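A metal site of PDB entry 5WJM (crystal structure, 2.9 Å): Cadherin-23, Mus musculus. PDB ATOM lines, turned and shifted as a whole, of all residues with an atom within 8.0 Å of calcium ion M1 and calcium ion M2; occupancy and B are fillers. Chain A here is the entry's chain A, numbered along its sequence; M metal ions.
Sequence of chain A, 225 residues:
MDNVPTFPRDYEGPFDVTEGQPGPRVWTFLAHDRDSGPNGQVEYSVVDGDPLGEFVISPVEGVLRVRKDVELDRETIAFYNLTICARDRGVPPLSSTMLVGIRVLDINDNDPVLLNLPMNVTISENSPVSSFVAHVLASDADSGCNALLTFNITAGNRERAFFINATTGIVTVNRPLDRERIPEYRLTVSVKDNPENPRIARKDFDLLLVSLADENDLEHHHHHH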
ATOM      1  N   GLU A 125      20.009 -12.395  27.004  1.00  0.00           N
ATOM      2  CA  GLU A 125      21.251 -12.373  27.791  1.00  0.00           C
ATOM      3  C   GLU A 125      22.314 -11.487  27.132  1.00  0.00           C
ATOM      4  O   GLU A 125      23.131 -10.848  27.814  1.00  0.00           O
ATOM      5  CB  GLU A 125      21.802 -13.781  28.074  1.00  0.00           C
ATOM      6  CG  GLU A 125      22.110 -14.674  26.866  1.00  0.00           C
ATOM      7  CD  GLU A 125      23.016 -15.860  27.194  1.00  0.00           C
ATOM      8  OE1 GLU A 125      23.796 -15.786  28.174  1.00  0.00           O
ATOM      9  OE2 GLU A 125      22.995 -16.882  26.457  1.00  0.00           O
ATOM     10  N   ASN A 126      22.262 -11.429  25.803  1.00  0.00           N
ATOM     11  CA  ASN A 126      23.134 -10.564  25.008  1.00  0.00           C
ATOM     12  C   ASN A 126      22.633  -9.130  24.891  1.00  0.00           C
ATOM     13  O   ASN A 126      23.183  -8.362  24.101  1.00  0.00           O
ATOM     14  CB  ASN A 126      23.317 -11.144  23.596  1.00  0.00           C
ATOM     15  CG  ASN A 126      23.949 -12.528  23.591  1.00  0.00           C
ATOM     16  OD1 ASN A 126      24.352 -13.073  24.629  1.00  0.00           O
ATOM     17  ND2 ASN A 126      24.027 -13.105  22.414  1.00  0.00           N
ATOM     18  N   LEU A 177      25.600  -9.011  30.493  1.00  0.00           N
ATOM     19  CA  LEU A 177      24.830 -10.046  31.162  1.00  0.00           C
ATOM     20  C   LEU A 177      25.213 -11.421  30.610  1.00  0.00           C
ATOM     21  O   LEU A 177      25.514 -11.537  29.424  1.00  0.00           O
ATOM     22  CB  LEU A 177      23.343  -9.791  30.900  1.00  0.00           C
ATOM     23  CG  LEU A 177      22.506  -8.921  31.848  1.00  0.00           C
ATOM     24  CD1 LEU A 177      23.221  -7.650  32.297  1.00  0.00           C
ATOM     25  CD2 LEU A 177      21.191  -8.577  31.173  1.00  0.00           C
ATOM     26  N   ASP A 178      25.206 -12.451  31.456  1.00  0.00           N
ATOM     27  CA  ASP A 178      25.325 -13.862  31.027  1.00  0.00           C
ATOM     28  C   ASP A 178      24.293 -14.700  31.771  1.00  0.00           C
ATOM     29  O   ASP A 178      24.142 -14.583  32.986  1.00  0.00           O
ATOM     30  CB  ASP A 178      26.752 -14.389  31.289  1.00  0.00           C
ATOM     31  CG  ASP A 178      27.094 -15.690  30.518  1.00  0.00           C
ATOM     32  OD1 ASP A 178      26.728 -15.866  29.330  1.00  0.00           O
ATOM     33  OD2 ASP A 178      27.801 -16.541  31.121  1.00  0.00           O
ATOM     34  N   ARG A 179      23.549 -15.522  31.033  1.00  0.00           N
ATOM     35  CA  ARG A 179      22.518 -16.357  31.638  1.00  0.00           C
ATOM     36  C   ARG A 179      23.129 -17.523  32.402  1.00  0.00           C
ATOM     37  O   ARG A 179      22.512 -18.056  33.312  1.00  0.00           O
ATOM     38  CB  ARG A 179      21.562 -16.907  30.584  1.00  0.00           C
ATOM     39  CG  ARG A 179      20.229 -17.373  31.167  1.00  0.00           C
ATOM     40  CD  ARG A 179      19.307 -17.941  30.086  1.00  0.00           C
ATOM     41  NE  ARG A 179      19.926 -19.119  29.479  1.00  0.00           N
ATOM     42  CZ  ARG A 179      19.993 -20.319  30.048  1.00  0.00           C
ATOM     43  NH1 ARG A 179      19.449 -20.551  31.241  1.00  0.00           N
ATOM     44  NH2 ARG A 179      20.612 -21.311  29.409  1.00  0.00           N
ATOM     45  N   GLU A 180      24.321 -17.919  32.017  1.00  0.00           N
ATOM     46  CA  GLU A 180      24.961 -19.077  32.617  1.00  0.00           C
ATOM     47  C   GLU A 180      25.579 -18.708  33.959  1.00  0.00           C
ATOM     48  O   GLU A 180      25.735 -19.574  34.816  1.00  0.00           O
ATOM     49  CB  GLU A 180      25.982 -19.704  31.655  1.00  0.00           C
ATOM     50  CG  GLU A 180      25.385 -20.399  30.419  1.00  0.00           C
ATOM     51  CD  GLU A 180      24.846 -19.435  29.353  1.00  0.00           C
ATOM     52  OE1 GLU A 180      23.828 -19.763  28.708  1.00  0.00           O
ATOM     53  OE2 GLU A 180      25.440 -18.344  29.137  1.00  0.00           O
ATOM     54  N   ARG A 181      25.927 -17.429  34.152  1.00  0.00           N
ATOM     55  CA  ARG A 181      26.295 -16.898  35.482  1.00  0.00           C
ATOM     56  C   ARG A 181      25.068 -16.629  36.329  1.00  0.00           C
ATOM     57  O   ARG A 181      24.931 -17.201  37.383  1.00  0.00           O
ATOM     58  CB  ARG A 181      27.078 -15.590  35.389  1.00  0.00           C
ATOM     59  CG  ARG A 181      28.460 -15.702  34.764  1.00  0.00           C
ATOM     60  CD  ARG A 181      29.180 -14.358  34.842  1.00  0.00           C
ATOM     61  NE  ARG A 181      29.180 -13.859  36.209  1.00  0.00           N
ATOM     62  CZ  ARG A 181      29.994 -14.290  37.182  1.00  0.00           C
ATOM     63  NH1 ARG A 181      29.886 -13.766  38.399  1.00  0.00           N
ATOM     64  NH2 ARG A 181      30.913 -15.232  36.958  1.00  0.00           N
ATOM     65  N   ALA A 213      16.564 -14.608  28.582  1.00  0.00           N
ATOM     66  CA  ALA A 213      16.390 -15.636  27.552  1.00  0.00           C
ATOM     67  C   ALA A 213      17.738 -16.191  27.043  1.00  0.00           C
ATOM     68  O   ALA A 213      18.688 -15.418  26.880  1.00  0.00           O
ATOM     69  CB  ALA A 213      15.615 -15.065  26.386  1.00  0.00           C
ATOM     70  N   ASP A 214      17.804 -17.484  26.758  1.00  0.00           N
ATOM     71  CA  ASP A 214      19.061 -18.088  26.284  1.00  0.00           C
ATOM     72  C   ASP A 214      19.451 -17.596  24.876  1.00  0.00           C
ATOM     73  O   ASP A 214      18.600 -17.199  24.085  1.00  0.00           O
ATOM     74  CB  ASP A 214      19.031 -19.632  26.310  1.00  0.00           C
ATOM     75  CG  ASP A 214      20.462 -20.271  26.285  1.00  0.00           C
ATOM     76  OD1 ASP A 214      21.379 -19.789  26.993  1.00  0.00           O
ATOM     77  OD2 ASP A 214      20.679 -21.267  25.575  1.00  0.00           O
ATOM     78  N   GLU A 215      20.771 -17.569  24.639  1.00  0.00           N
ATOM     79  CA  GLU A 215      21.392 -17.347  23.324  1.00  0.00           C
ATOM     80  C   GLU A 215      22.673 -18.205  23.228  1.00  0.00           C
ATOM     81  O   GLU A 215      22.999 -18.958  24.164  1.00  0.00           O
ATOM     82  CB  GLU A 215      21.733 -15.849  23.133  1.00  0.00           C
ATOM     83  CG  GLU A 215      20.572 -14.856  23.177  1.00  0.00           C
ATOM     84  CD  GLU A 215      19.695 -14.880  21.928  1.00  0.00           C
ATOM     85  OE1 GLU A 215      19.417 -15.980  21.389  1.00  0.00           O
ATOM     86  OE2 GLU A 215      19.258 -13.797  21.476  1.00  0.00           O
ATOM     87  N   ASN A 216      23.398 -18.073  22.118  1.00  0.00           N
ATOM     88  CA  ASN A 216      24.680 -18.769  21.920  1.00  0.00           C
ATOM     89  C   ASN A 216      25.779 -18.334  22.891  1.00  0.00           C
ATOM     90  O   ASN A 216      25.560 -17.424  23.719  1.00  0.00           O
ATOM     91  CB  ASN A 216      25.186 -18.590  20.481  1.00  0.00           C
ATOM     92  CG  ASN A 216      24.332 -19.324  19.472  1.00  0.00           C
ATOM     93  OD1 ASN A 216      23.366 -19.994  19.834  1.00  0.00           O
ATOM     94  ND2 ASN A 216      24.680 -19.193  18.186  1.00  0.00           N
ATOM     95  N   ASP A 217      26.922 -19.030  22.798  1.00  0.00           N
ATOM     96  CA  ASP A 217      28.121 -18.771  23.600  1.00  0.00           C
ATOM     97  C   ASP A 217      29.373 -19.142  22.791  1.00  0.00           C
ATOM     98  O   ASP A 217      30.129 -18.274  22.368  1.00  0.00           O
ATOM     99  CB  ASP A 217      28.079 -19.600  24.902  1.00  0.00           C
ATOM    100  CG  ASP A 217      26.821 -19.316  25.761  1.00  0.00           C
ATOM    101  OD1 ASP A 217      25.769 -19.964  25.554  1.00  0.00           O
ATOM    102  OD2 ASP A 217      26.877 -18.428  26.646  1.00  0.00           O
HETATM  103 CA    CA M   1      26.075 -16.209  27.158  1.00  0.00          CA
HETATM  104 CA    CA M   2      23.634 -19.345  26.418  1.00  0.00          CA
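The side-chain carboxylate of Glu 180 sits close to the guanidinium group of Arg 179 (3.6 Å).
The side-chain carboxylate (OD2) of Asp 214 is in salt-bridge range of the guanidinium group (NH2) of Arg 179.
OE1 of Glu 125 sits close to N of Arg 179, 2.9 Å away.
N of Glu 125 is in hydrogen-bond range of O of Ala 213 (3.3 Å).
Residues that only touch calcium ion M1: Asn 216 (3.7 Å).
Five residues have an atom within 4 Å of calcium ion M1: Glu 125, Asp 178, Glu 180, Asn 216 and Asp 217.
O of Asn 216 touches calcium ion M2, 3.8 Å away.
Along chain A the residues within 4 Å of calcium ion M2 span positions 125 to 217.
The nearest printed residue that does not touch calcium ion M2 is Arg 179 (4.7 Å).
Calcium ion M1 is bound by OD1 of Asp 178 (2.3 Å).
Calcium ion M1 is bound by OD2 of Asp 217.
Calcium ion M1 is bound by the side-chain carboxylate (OE1) of Glu 125 (2.5 Å).
Slightly farther from calcium ion M1 lies OE2 of Glu 180 (3.0 Å).
Calcium ion M2 is bound by OE1 of Glu 180 (2.3 Å), OD1 of Asp 214 (2.4 Å), O of Glu 215 (2.4 Å), OD1 of Asp 217 (2.4 Å) and OE2 of Glu 125 (2.5 Å).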
